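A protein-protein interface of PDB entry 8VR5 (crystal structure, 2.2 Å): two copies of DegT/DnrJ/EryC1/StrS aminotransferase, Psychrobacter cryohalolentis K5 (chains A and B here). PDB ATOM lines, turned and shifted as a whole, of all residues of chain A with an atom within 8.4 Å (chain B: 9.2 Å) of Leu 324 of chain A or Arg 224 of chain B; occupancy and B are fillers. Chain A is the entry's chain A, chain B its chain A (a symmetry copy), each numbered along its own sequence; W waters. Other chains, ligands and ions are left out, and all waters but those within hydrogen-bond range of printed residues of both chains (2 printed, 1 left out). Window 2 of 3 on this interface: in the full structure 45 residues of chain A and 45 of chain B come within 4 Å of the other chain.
ND2 of Asn 330 of chain A sits at hydrogen-bond distance from O of Phe 325 of chain A. The side-chain amino group (NZ) of Lys 93 of chain A lies within salt-bridge range of the side-chain carboxylate (OE1) of Glu 88 of chain A (3.1 Å). OE1 of Glu 222 of chain B is in salt-bridge range of NE of Arg 224 of chain B, 3.0 Å away. The side-chain carboxylate of Glu 88 of chain A is in hydrogen-bond range of the backbone NH of Ala 94 of chain A (2.8 Å). The backbone carbonyl oxygen of Gly 213 of chain B sits at hydrogen-bond distance from the backbone NH of Arg 224 of chain B (2.9 Å).
Among the printed residues, pairs that only touch across the chains: Ala 81 of chain A with Phe 223 of chain B (3.8 Å), Asn 85 of chain A with His 212 of chain B (3.6 Å), Asn 85 of chain A with Ile 226 of chain B (3.4 Å), Asn 85 of chain A with Gly 227 of chain B (3.6 Å), Glu 88 of chain A with Ile 226 of chain B (3.7 Å), Leu 322 of chain A with Phe 223 of chain B (3.99 Å), Leu 324 of chain A with Phe 223 of chain B (3.9 Å), Leu 324 of chain A with Arg 224 of chain B (3.7 Å), Leu 324 of chain A with Cys 225 of chain B (3.9 Å) and Phe 325 of chain A with Ile 226 of chain B (3.8 Å).
Leu 324 of chain A touches just these residues of chain B: Phe 223 (3.9 Å), Arg 224 (3.7 Å) and Cys 225 (3.9 Å). Arg 224 of chain B touches just one residue of chain A: Leu 324 (3.7 Å). Phe 325 of chain A touches just one residue of chain B: Ile 226. Cys 225 of chain B touches just one residue of chain A: Leu 324. Of the printed residues of chain A, Ile 226 of chain B touches Asn 85 (3.4 Å), Glu 88 (3.7 Å) and Phe 325 (3.8 Å). Printed residues of chain A within 4 Å of Phe 223 of chain B: Ala 81, Leu 322 and Leu 324. Thr 331 of chain A touches none of the printed residues of chain B. Met 214 of chain B touches none of the printed residues of chain A.
Of the 19 printed residues of chain A, 6 touch a printed residue of chain B. Hydrophobic or aromatic side chains of chain A within 4 Å of the printed part of chain B: Ala 81, Leu 322, Leu 324 and Phe 325. Printed residues of chain B that touch a printed residue of chain A: His 212, Phe 223, Arg 224, Cys 225, Ile 226 and Gly 227. Hydrophobic or aromatic side chains of chain B within 4 Å of the printed part of chain A: Phe 223 and Ile 226. Among the printed residues, no Asp or Glu carboxylate lies within 4 Å of a Lys or Arg side-chain nitrogen of the other chain.
No position is printed for both chains. Of the 10 pairs that touch across the chains among the printed residues, none has its exchanged pair printed and touching as well.
Water W1 lies within hydrogen-bond range of O of Phe 223 of chain B (2.6 Å) and O of Leu 322 of chain A (2.7 Å). Water W2 lies within hydrogen-bond range of O of His 212 of chain B (3.0 Å), ND2 of Asn 85 of chain A (3.0 Å) and O of Cys 225 of chain B (3.1 Å).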
ATOM      1  N   ALA A  81     -25.431 -16.039  28.004  1.00  0.00           N
ATOM      2  CA  ALA A  81     -25.119 -14.633  28.086  1.00  0.00           C
ATOM      3  C   ALA A  81     -26.308 -13.831  28.587  1.00  0.00           C
ATOM      4  O   ALA A  81     -26.117 -12.752  29.131  1.00  0.00           O
ATOM      5  CB  ALA A  81     -24.719 -14.164  26.719  1.00  0.00           C
ATOM      6  N   ALA A  84     -26.233 -12.230  32.283  1.00  0.00           N
ATOM      7  CA  ALA A  84     -25.518 -10.978  32.473  1.00  0.00           C
ATOM      8  C   ALA A  84     -26.098  -9.869  31.595  1.00  0.00           C
ATOM      9  O   ALA A  84     -26.190  -8.735  32.046  1.00  0.00           O
ATOM     10  CB  ALA A  84     -24.038 -11.128  32.176  1.00  0.00           C
ATOM     11  N   ASN A  85     -26.387 -10.173  30.324  1.00  0.00           N
ATOM     12  CA  ASN A  85     -26.972  -9.207  29.419  1.00  0.00           C
ATOM     13  C   ASN A  85     -28.182  -8.553  30.049  1.00  0.00           C
ATOM     14  O   ASN A  85     -28.364  -7.342  29.920  1.00  0.00           O
ATOM     15  CB  ASN A  85     -27.447  -9.825  28.108  1.00  0.00           C
ATOM     16  CG  ASN A  85     -26.324 -10.142  27.147  1.00  0.00           C
ATOM     17  OD1 ASN A  85     -25.189  -9.709  27.334  1.00  0.00           O
ATOM     18  ND2 ASN A  85     -26.641 -10.870  26.097  1.00  0.00           N
ATOM     19  N   GLU A  88     -27.616  -5.834  32.457  1.00  0.00           N
ATOM     20  CA  GLU A  88     -27.099  -4.603  31.892  1.00  0.00           C
ATOM     21  C   GLU A  88     -28.150  -3.893  31.037  1.00  0.00           C
ATOM     22  O   GLU A  88     -28.078  -2.673  30.918  1.00  0.00           O
ATOM     23  CB  GLU A  88     -25.817  -4.857  31.101  1.00  0.00           C
ATOM     24  CG  GLU A  88     -24.714  -5.449  31.955  1.00  0.00           C
ATOM     25  CD  GLU A  88     -23.509  -4.572  32.261  1.00  0.00           C
ATOM     26  OE1 GLU A  88     -23.298  -3.602  31.554  1.00  0.00           O
ATOM     27  OE2 GLU A  88     -22.804  -4.867  33.230  1.00  0.00           O
ATOM     28  N   LYS A  93     -25.303  -3.078  36.550  1.00  0.00           N
ATOM     29  CA  LYS A  93     -24.029  -3.625  36.143  1.00  0.00           C
ATOM     30  C   LYS A  93     -23.921  -5.068  36.627  1.00  0.00           C
ATOM     31  O   LYS A  93     -24.289  -5.426  37.747  1.00  0.00           O
ATOM     32  CB  LYS A  93     -22.911  -2.759  36.723  1.00  0.00           C
ATOM     33  CG  LYS A  93     -22.964  -1.288  36.312  1.00  0.00           C
ATOM     34  CD  LYS A  93     -22.777  -1.009  34.839  1.00  0.00           C
ATOM     35  CE  LYS A  93     -21.502  -1.550  34.238  1.00  0.00           C
ATOM     36  NZ  LYS A  93     -21.491  -1.359  32.761  1.00  0.00           N
ATOM     37  N   ALA A  94     -23.399  -5.900  35.753  1.00  0.00           N
ATOM     38  CA  ALA A  94     -23.299  -7.304  36.057  1.00  0.00           C
ATOM     39  C   ALA A  94     -21.938  -7.514  36.693  1.00  0.00           C
ATOM     40  O   ALA A  94     -20.950  -7.237  36.033  1.00  0.00           O
ATOM     41  CB  ALA A  94     -23.474  -8.089  34.785  1.00  0.00           C
ATOM     42  N   ILE A  96     -19.328 -10.203  38.102  1.00  0.00           N
ATOM     43  CA  ILE A  96     -19.187 -11.611  37.832  1.00  0.00           C
ATOM     44  C   ILE A  96     -18.441 -12.296  38.960  1.00  0.00           C
ATOM     45  O   ILE A  96     -17.429 -11.804  39.430  1.00  0.00           O
ATOM     46  CB  ILE A  96     -18.502 -11.881  36.489  1.00  0.00           C
ATOM     47  CG1 ILE A  96     -19.198 -11.123  35.359  1.00  0.00           C
ATOM     48  CG2 ILE A  96     -18.432 -13.381  36.231  1.00  0.00           C
ATOM     49  CD1 ILE A  96     -18.381 -11.058  34.085  1.00  0.00           C
ATOM     50  N   SER A 318     -18.444 -18.319  29.122  1.00  0.00           N
ATOM     51  CA  SER A 318     -17.795 -17.515  30.161  1.00  0.00           C
ATOM     52  C   SER A 318     -18.078 -16.024  30.010  1.00  0.00           C
ATOM     53  O   SER A 318     -17.717 -15.425  29.002  1.00  0.00           O
ATOM     54  CB  SER A 318     -16.311 -17.674  30.153  1.00  0.00           C
ATOM     55  OG  SER A 318     -15.686 -16.729  31.022  1.00  0.00           O
ATOM     56  N   MET A 319     -18.739 -15.422  31.000  1.00  0.00           N
ATOM     57  CA  MET A 319     -19.189 -14.043  30.857  1.00  0.00           C
ATOM     58  C   MET A 319     -17.950 -13.124  30.811  1.00  0.00           C
ATOM     59  O   MET A 319     -17.949 -12.127  30.102  1.00  0.00           O
ATOM     60  CB  MET A 319     -20.109 -13.617  32.024  1.00  0.00           C
ATOM     61  CG  MET A 319     -21.452 -14.342  32.141  1.00  0.00           C
ATOM     62  SD  MET A 319     -22.516 -14.241  30.699  1.00  0.00           S
ATOM     63  CE  MET A 319     -21.917 -15.641  29.760  1.00  0.00           C
ATOM     64  N   SER A 320     -16.904 -13.434  31.609  1.00  0.00           N
ATOM     65  CA  SER A 320     -15.701 -12.625  31.649  1.00  0.00           C
ATOM     66  C   SER A 320     -15.041 -12.646  30.271  1.00  0.00           C
ATOM     67  O   SER A 320     -14.617 -11.607  29.782  1.00  0.00           O
ATOM     68  CB  SER A 320     -14.778 -13.039  32.762  1.00  0.00           C
ATOM     69  OG  SER A 320     -14.553 -14.433  32.778  1.00  0.00           O
ATOM     70  N   GLU A 321     -15.055 -13.806  29.614  1.00  0.00           N
ATOM     71  CA  GLU A 321     -14.395 -13.950  28.331  1.00  0.00           C
ATOM     72  C   GLU A 321     -15.147 -13.204  27.229  1.00  0.00           C
ATOM     73  O   GLU A 321     -14.535 -12.833  26.230  1.00  0.00           O
ATOM     74  CB  GLU A 321     -14.249 -15.409  27.921  1.00  0.00           C
ATOM     75  CG  GLU A 321     -13.228 -16.166  28.734  1.00  0.00           C
ATOM     76  CD  GLU A 321     -11.806 -15.646  28.656  1.00  0.00           C
ATOM     77  OE1 GLU A 321     -11.226 -15.365  29.706  1.00  0.00           O
ATOM     78  OE2 GLU A 321     -11.303 -15.507  27.530  1.00  0.00           O
ATOM     79  N   LEU A 322     -16.455 -12.982  27.372  1.00  0.00           N
ATOM     80  CA  LEU A 322     -17.146 -12.274  26.308  1.00  0.00           C
ATOM     81  C   LEU A 322     -16.675 -10.809  26.219  1.00  0.00           C
ATOM     82  O   LEU A 322     -16.833 -10.191  25.167  1.00  0.00           O
ATOM     83  CB  LEU A 322     -18.659 -12.354  26.545  1.00  0.00           C
ATOM     84  CG  LEU A 322     -19.277 -13.752  26.492  1.00  0.00           C
ATOM     85  CD1 LEU A 322     -20.762 -13.707  26.807  1.00  0.00           C
ATOM     86  CD2 LEU A 322     -19.049 -14.412  25.142  1.00  0.00           C
ATOM     87  N   LYS A 323     -16.142 -10.243  27.327  1.00  0.00           N
ATOM     88  CA  LYS A 323     -15.670  -8.856  27.395  1.00  0.00           C
ATOM     89  C   LYS A 323     -16.810  -7.870  27.163  1.00  0.00           C
ATOM     90  O   LYS A 323     -16.622  -6.905  26.436  1.00  0.00           O
ATOM     91  CB  LYS A 323     -14.619  -8.510  26.325  1.00  0.00           C
ATOM     92  CG  LYS A 323     -13.343  -9.340  26.297  1.00  0.00           C
ATOM     93  CD  LYS A 323     -12.703  -9.328  27.626  1.00  0.00           C
ATOM     94  CE  LYS A 323     -11.268  -9.787  27.618  1.00  0.00           C
ATOM     95  NZ  LYS A 323     -10.703  -9.599  28.982  1.00  0.00           N
ATOM     96  N   LEU A 324     -17.984  -8.104  27.762  1.00  0.00           N
ATOM     97  CA  LEU A 324     -19.130  -7.214  27.598  1.00  0.00           C
ATOM     98  C   LEU A 324     -19.497  -6.558  28.926  1.00  0.00           C
ATOM     99  O   LEU A 324     -20.239  -5.585  28.938  1.00  0.00           O
ATOM    100  CB  LEU A 324     -20.320  -8.016  27.060  1.00  0.00           C
ATOM    101  CG  LEU A 324     -20.143  -8.652  25.678  1.00  0.00           C
ATOM    102  CD1 LEU A 324     -21.376  -9.446  25.299  1.00  0.00           C
ATOM    103  CD2 LEU A 324     -19.838  -7.607  24.620  1.00  0.00           C
ATOM    104  N   PHE A 325     -18.978  -7.096  30.033  1.00  0.00           N
ATOM    105  CA  PHE A 325     -19.431  -6.744  31.370  1.00  0.00           C
ATOM    106  C   PHE A 325     -18.214  -6.160  32.074  1.00  0.00           C
ATOM    107  O   PHE A 325     -17.412  -6.863  32.690  1.00  0.00           O
ATOM    108  CB  PHE A 325     -20.076  -7.966  32.042  1.00  0.00           C
ATOM    109  CG  PHE A 325     -21.039  -8.694  31.152  1.00  0.00           C
ATOM    110  CD1 PHE A 325     -22.210  -8.080  30.725  1.00  0.00           C
ATOM    111  CD2 PHE A 325     -20.742  -9.944  30.654  1.00  0.00           C
ATOM    112  CE1 PHE A 325     -23.086  -8.715  29.863  1.00  0.00           C
ATOM    113  CE2 PHE A 325     -21.606 -10.575  29.777  1.00  0.00           C
ATOM    114  CZ  PHE A 325     -22.775  -9.954  29.365  1.00  0.00           C
ATOM    115  N   ASN A 326     -18.040  -4.854  31.892  1.00  0.00           N
ATOM    116  CA  ASN A 326     -16.725  -4.263  32.033  1.00  0.00           C
ATOM    117  C   ASN A 326     -16.639  -3.372  33.264  1.00  0.00           C
ATOM    118  O   ASN A 326     -15.756  -2.541  33.331  1.00  0.00           O
ATOM    119  CB  ASN A 326     -16.336  -3.538  30.741  1.00  0.00           C
ATOM    120  CG  ASN A 326     -16.095  -4.493  29.583  1.00  0.00           C
ATOM    121  OD1 ASN A 326     -15.248  -5.385  29.640  1.00  0.00           O
ATOM    122  ND2 ASN A 326     -16.860  -4.323  28.528  1.00  0.00           N
ATOM    123  N   HIS A 327     -17.494  -3.566  34.270  1.00  0.00           N
ATOM    124  CA  HIS A 327     -17.258  -2.922  35.549  1.00  0.00           C
ATOM    125  C   HIS A 327     -15.847  -3.268  35.992  1.00  0.00           C
ATOM    126  O   HIS A 327     -15.390  -4.380  35.788  1.00  0.00           O
ATOM    127  CB  HIS A 327     -18.283  -3.369  36.589  1.00  0.00           C
ATOM    128  CG  HIS A 327     -18.334  -2.605  37.863  1.00  0.00           C
ATOM    129  ND1 HIS A 327     -17.549  -2.943  38.947  1.00  0.00           N
ATOM    130  CD2 HIS A 327     -19.131  -1.605  38.271  1.00  0.00           C
ATOM    131  CE1 HIS A 327     -17.863  -2.168  39.973  1.00  0.00           C
ATOM    132  NE2 HIS A 327     -18.799  -1.326  39.579  1.00  0.00           N
ATOM    133  N   ASN A 330     -14.948  -6.395  37.622  1.00  0.00           N
ATOM    134  CA  ASN A 330     -14.740  -7.594  36.839  1.00  0.00           C
ATOM    135  C   ASN A 330     -13.339  -7.604  36.223  1.00  0.00           C
ATOM    136  O   ASN A 330     -12.703  -8.650  36.211  1.00  0.00           O
ATOM    137  CB  ASN A 330     -15.794  -7.760  35.742  1.00  0.00           C
ATOM    138  CG  ASN A 330     -17.207  -7.860  36.277  1.00  0.00           C
ATOM    139  OD1 ASN A 330     -17.420  -8.311  37.398  1.00  0.00           O
ATOM    140  ND2 ASN A 330     -18.169  -7.476  35.440  1.00  0.00           N
ATOM    141  N   THR A 331     -12.866  -6.461  35.695  1.00  0.00           N
ATOM    142  CA  THR A 331     -11.576  -6.398  35.006  1.00  0.00           C
ATOM    143  C   THR A 331     -10.423  -6.585  35.994  1.00  0.00           C
ATOM    144  O   THR A 331      -9.362  -7.031  35.596  1.00  0.00           O
ATOM    145  CB  THR A 331     -11.399  -5.122  34.161  1.00  0.00           C
ATOM    146  OG1 THR A 331     -11.652  -3.987  34.977  1.00  0.00           O
ATOM    147  CG2 THR A 331     -12.324  -5.030  32.965  1.00  0.00           C
ATOM    148  N   GLU B 204     -29.109  -4.297  11.381  1.00  0.00           N
ATOM    149  CA  GLU B 204     -28.137  -5.199  11.979  1.00  0.00           C
ATOM    150  C   GLU B 204     -28.140  -5.015  13.497  1.00  0.00           C
ATOM    151  O   GLU B 204     -28.023  -5.977  14.229  1.00  0.00           O
ATOM    152  CB  GLU B 204     -26.698  -5.060  11.441  1.00  0.00           C
ATOM    153  CG  GLU B 204     -26.457  -5.586  10.008  1.00  0.00           C
ATOM    154  CD  GLU B 204     -26.739  -7.045   9.586  1.00  0.00           C
ATOM    155  OE1 GLU B 204     -26.848  -7.275   8.337  1.00  0.00           O
ATOM    156  OE2 GLU B 204     -26.807  -7.999  10.451  1.00  0.00           O
ATOM    157  N   LEU B 208     -29.155  -7.813  16.384  1.00  0.00           N
ATOM    158  CA  LEU B 208     -28.348  -8.178  17.538  1.00  0.00           C
ATOM    159  C   LEU B 208     -29.174  -8.066  18.822  1.00  0.00           C
ATOM    160  O   LEU B 208     -29.151  -8.963  19.662  1.00  0.00           O
ATOM    161  CB  LEU B 208     -27.131  -7.266  17.620  1.00  0.00           C
ATOM    162  CG  LEU B 208     -26.025  -7.518  16.588  1.00  0.00           C
ATOM    163  CD1 LEU B 208     -25.046  -6.348  16.526  1.00  0.00           C
ATOM    164  CD2 LEU B 208     -25.284  -8.794  16.894  1.00  0.00           C
ATOM    165  N   LEU B 209     -29.914  -6.967  18.972  1.00  0.00           N
ATOM    166  CA  LEU B 209     -30.677  -6.701  20.183  1.00  0.00           C
ATOM    167  C   LEU B 209     -31.793  -7.722  20.368  1.00  0.00           C
ATOM    168  O   LEU B 209     -32.094  -8.077  21.506  1.00  0.00           O
ATOM    169  CB  LEU B 209     -31.263  -5.293  20.114  1.00  0.00           C
ATOM    170  CG  LEU B 209     -30.259  -4.180  20.393  1.00  0.00           C
ATOM    171  CD1 LEU B 209     -30.926  -2.835  20.252  1.00  0.00           C
ATOM    172  CD2 LEU B 209     -29.612  -4.334  21.761  1.00  0.00           C
ATOM    173  N   SER B 211     -31.718 -10.918  19.800  1.00  0.00           N
ATOM    174  CA  SER B 211     -31.303 -12.237  20.232  1.00  0.00           C
ATOM    175  C   SER B 211     -29.911 -12.249  20.875  1.00  0.00           C
ATOM    176  O   SER B 211     -28.987 -12.870  20.342  1.00  0.00           O
ATOM    177  CB  SER B 211     -31.358 -13.238  19.121  1.00  0.00           C
ATOM    178  OG  SER B 211     -31.197 -14.551  19.698  1.00  0.00           O
ATOM    179  N   HIS B 212     -29.814 -11.610  22.048  1.00  0.00           N
ATOM    180  CA  HIS B 212     -28.680 -11.729  22.942  1.00  0.00           C
ATOM    181  C   HIS B 212     -27.381 -11.303  22.276  1.00  0.00           C
ATOM    182  O   HIS B 212     -26.316 -11.782  22.645  1.00  0.00           O
ATOM    183  CB  HIS B 212     -28.541 -13.174  23.390  1.00  0.00           C
ATOM    184  CG  HIS B 212     -29.802 -13.689  23.982  1.00  0.00           C
ATOM    185  ND1 HIS B 212     -30.339 -13.140  25.135  1.00  0.00           N
ATOM    186  CD2 HIS B 212     -30.649 -14.687  23.572  1.00  0.00           C
ATOM    187  CE1 HIS B 212     -31.468 -13.790  25.425  1.00  0.00           C
ATOM    188  NE2 HIS B 212     -31.667 -14.769  24.507  1.00  0.00           N
ATOM    189  N   GLY B 213     -27.466 -10.381  21.332  1.00  0.00           N
ATOM    190  CA  GLY B 213     -26.279  -9.929  20.633  1.00  0.00           C
ATOM    191  C   GLY B 213     -25.574 -11.016  19.825  1.00  0.00           C
ATOM    192  O   GLY B 213     -24.390 -10.865  19.533  1.00  0.00           O
ATOM    193  N   MET B 214     -26.303 -12.051  19.384  1.00  0.00           N
ATOM    194  CA  MET B 214     -25.708 -13.156  18.645  1.00  0.00           C
ATOM    195  C   MET B 214     -25.537 -12.774  17.171  1.00  0.00           C
ATOM    196  O   MET B 214     -26.421 -12.142  16.602  1.00  0.00           O
ATOM    197  CB  MET B 214     -26.610 -14.389  18.757  1.00  0.00           C
ATOM    198  CG  MET B 214     -26.614 -15.010  20.146  1.00  0.00           C
ATOM    199  SD  MET B 214     -28.060 -16.095  20.493  1.00  0.00           S
ATOM    200  CE  MET B 214     -27.782 -17.450  19.353  1.00  0.00           C
ATOM    201  N   MET B 215     -24.398 -13.152  16.562  1.00  0.00           N
ATOM    202  CA  MET B 215     -24.226 -13.184  15.108  1.00  0.00           C
ATOM    203  C   MET B 215     -23.238 -14.283  14.707  1.00  0.00           C
ATOM    204  O   MET B 215     -22.582 -14.866  15.561  1.00  0.00           O
ATOM    205  CB  MET B 215     -23.727 -11.851  14.556  1.00  0.00           C
ATOM    206  CG  MET B 215     -22.450 -11.345  15.183  1.00  0.00           C
ATOM    207  SD  MET B 215     -21.637 -10.234  14.021  1.00  0.00           S
ATOM    208  CE  MET B 215     -22.939  -9.034  13.700  1.00  0.00           C
ATOM    209  N   ARG B 216     -23.163 -14.567  13.396  1.00  0.00           N
ATOM    210  CA  ARG B 216     -22.342 -15.639  12.832  1.00  0.00           C
ATOM    211  C   ARG B 216     -20.908 -15.157  12.643  1.00  0.00           C
ATOM    212  O   ARG B 216     -20.694 -14.167  11.957  1.00  0.00           O
ATOM    213  CB  ARG B 216     -22.832 -16.056  11.441  1.00  0.00           C
ATOM    214  CG  ARG B 216     -24.315 -16.396  11.357  1.00  0.00           C
ATOM    215  CD  ARG B 216     -24.978 -15.849  10.094  1.00  0.00           C
ATOM    216  NE  ARG B 216     -26.441 -15.758  10.137  1.00  0.00           N
ATOM    217  CZ  ARG B 216     -27.151 -14.803  10.749  1.00  0.00           C
ATOM    218  NH1 ARG B 216     -26.562 -13.831  11.430  1.00  0.00           N
ATOM    219  NH2 ARG B 216     -28.472 -14.823  10.680  1.00  0.00           N
ATOM    220  N   GLY B 217     -19.938 -15.866  13.236  1.00  0.00           N
ATOM    221  CA  GLY B 217     -18.519 -15.629  12.986  1.00  0.00           C
ATOM    222  C   GLY B 217     -17.802 -16.888  12.487  1.00  0.00           C
ATOM    223  O   GLY B 217     -18.367 -17.982  12.513  1.00  0.00           O
ATOM    224  N   GLU B 218     -16.538 -16.734  12.066  1.00  0.00           N
ATOM    225  CA  GLU B 218     -15.822 -17.768  11.328  1.00  0.00           C
ATOM    226  C   GLU B 218     -15.873 -19.109  12.075  1.00  0.00           C
ATOM    227  O   GLU B 218     -16.205 -20.119  11.472  1.00  0.00           O
ATOM    228  CB  GLU B 218     -14.402 -17.291  10.983  1.00  0.00           C
ATOM    229  CG  GLU B 218     -14.346 -16.355   9.761  1.00  0.00           C
ATOM    230  CD  GLU B 218     -12.987 -15.733   9.428  1.00  0.00           C
ATOM    231  OE1 GLU B 218     -12.617 -14.718  10.066  1.00  0.00           O
ATOM    232  OE2 GLU B 218     -12.281 -16.259   8.534  1.00  0.00           O
ATOM    233  N   GLY B 220     -18.016 -19.921  14.487  1.00  0.00           N
ATOM    234  CA  GLY B 220     -19.316 -20.146  15.106  1.00  0.00           C
ATOM    235  C   GLY B 220     -20.034 -18.871  15.561  1.00  0.00           C
ATOM    236  O   GLY B 220     -19.728 -17.762  15.128  1.00  0.00           O
ATOM    237  N   ILE B 221     -21.047 -19.072  16.414  1.00  0.00           N
ATOM    238  CA  ILE B 221     -21.891 -18.008  16.946  1.00  0.00           C
ATOM    239  C   ILE B 221     -21.049 -17.137  17.874  1.00  0.00           C
ATOM    240  O   ILE B 221     -20.384 -17.657  18.753  1.00  0.00           O
ATOM    241  CB  ILE B 221     -23.149 -18.599  17.639  1.00  0.00           C
ATOM    242  CG1 ILE B 221     -24.424 -18.394  16.807  1.00  0.00           C
ATOM    243  CG2 ILE B 221     -23.334 -18.066  19.054  1.00  0.00           C
ATOM    244  CD1 ILE B 221     -24.615 -19.376  15.672  1.00  0.00           C
ATOM    245  N   GLU B 222     -21.080 -15.816  17.651  1.00  0.00           N
ATOM    246  CA  GLU B 222     -20.382 -14.859  18.497  1.00  0.00           C
ATOM    247  C   GLU B 222     -21.374 -13.957  19.250  1.00  0.00           C
ATOM    248  O   GLU B 222     -22.456 -13.637  18.783  1.00  0.00           O
ATOM    249  CB  GLU B 222     -19.430 -14.013  17.641  1.00  0.00           C
ATOM    250  CG  GLU B 222     -18.114 -14.712  17.269  1.00  0.00           C
ATOM    251  CD  GLU B 222     -17.263 -14.005  16.220  1.00  0.00           C
ATOM    252  OE1 GLU B 222     -17.613 -12.860  15.829  1.00  0.00           O
ATOM    253  OE2 GLU B 222     -16.255 -14.601  15.777  1.00  0.00           O
ATOM    254  N   PHE B 223     -20.954 -13.497  20.422  1.00  0.00           N
ATOM    255  CA  PHE B 223     -21.741 -12.590  21.238  1.00  0.00           C
ATOM    256  C   PHE B 223     -21.095 -11.203  21.229  1.00  0.00           C
ATOM    257  O   PHE B 223     -20.128 -10.950  21.948  1.00  0.00           O
ATOM    258  CB  PHE B 223     -21.899 -13.168  22.644  1.00  0.00           C
ATOM    259  CG  PHE B 223     -22.720 -14.432  22.699  1.00  0.00           C
ATOM    260  CD1 PHE B 223     -24.060 -14.389  23.034  1.00  0.00           C
ATOM    261  CD2 PHE B 223     -22.144 -15.658  22.459  1.00  0.00           C
ATOM    262  CE1 PHE B 223     -24.828 -15.536  23.072  1.00  0.00           C
ATOM    263  CE2 PHE B 223     -22.898 -16.823  22.520  1.00  0.00           C
ATOM    264  CZ  PHE B 223     -24.244 -16.756  22.818  1.00  0.00           C
ATOM    265  N   ARG B 224     -21.649 -10.320  20.389  1.00  0.00           N
ATOM    266  CA  ARG B 224     -21.016  -9.060  20.072  1.00  0.00           C
ATOM    267  C   ARG B 224     -21.479  -7.916  20.970  1.00  0.00           C
ATOM    268  O   ARG B 224     -20.771  -6.923  21.058  1.00  0.00           O
ATOM    269  CB  ARG B 224     -21.274  -8.689  18.611  1.00  0.00           C
ATOM    270  CG  ARG B 224     -20.547  -9.588  17.622  1.00  0.00           C
ATOM    271  CD  ARG B 224     -19.095  -9.849  18.010  1.00  0.00           C
ATOM    272  NE  ARG B 224     -18.296 -10.142  16.838  1.00  0.00           N
ATOM    273  CZ  ARG B 224     -18.123  -9.288  15.837  1.00  0.00           C
ATOM    274  NH1 ARG B 224     -18.653  -8.076  15.907  1.00  0.00           N
ATOM    275  NH2 ARG B 224     -17.409  -9.644  14.781  1.00  0.00           N
ATOM    276  N   CYS B 225     -22.652  -8.014  21.601  1.00  0.00           N
ATOM    277  CA  CYS B 225     -23.112  -6.945  22.474  1.00  0.00           C
ATOM    278  C   CYS B 225     -24.206  -7.465  23.387  1.00  0.00           C
ATOM    279  O   CYS B 225     -24.698  -8.540  23.146  1.00  0.00           O
ATOM    280  CB  CYS B 225     -23.647  -5.767  21.666  1.00  0.00           C
ATOM    281  SG  CYS B 225     -25.033  -6.201  20.564  1.00  0.00           S
ATOM    282  N   ILE B 226     -24.604  -6.690  24.402  1.00  0.00           N
ATOM    283  CA  ILE B 226     -25.734  -7.066  25.226  1.00  0.00           C
ATOM    284  C   ILE B 226     -27.017  -6.943  24.394  1.00  0.00           C
ATOM    285  O   ILE B 226     -27.146  -6.103  23.526  1.00  0.00           O
ATOM    286  CB  ILE B 226     -25.767  -6.237  26.527  1.00  0.00           C
ATOM    287  CG1 ILE B 226     -26.146  -4.778  26.284  1.00  0.00           C
ATOM    288  CG2 ILE B 226     -24.426  -6.325  27.240  1.00  0.00           C
ATOM    289  CD1 ILE B 226     -26.363  -3.973  27.567  1.00  0.00           C
ATOM    290  N   GLY B 227     -27.981  -7.822  24.639  1.00  0.00           N
ATOM    291  CA  GLY B 227     -29.279  -7.734  23.990  1.00  0.00           C
ATOM    292  C   GLY B 227     -30.353  -8.436  24.819  1.00  0.00           C
ATOM    293  O   GLY B 227     -30.120  -8.763  25.984  1.00  0.00           O
HETATM  294  O   HOH W   1     -17.731 -11.327  22.908  1.00  0.00           O
HETATM  295  O   HOH W   2     -24.137 -11.194  24.545  1.00  0.00           O
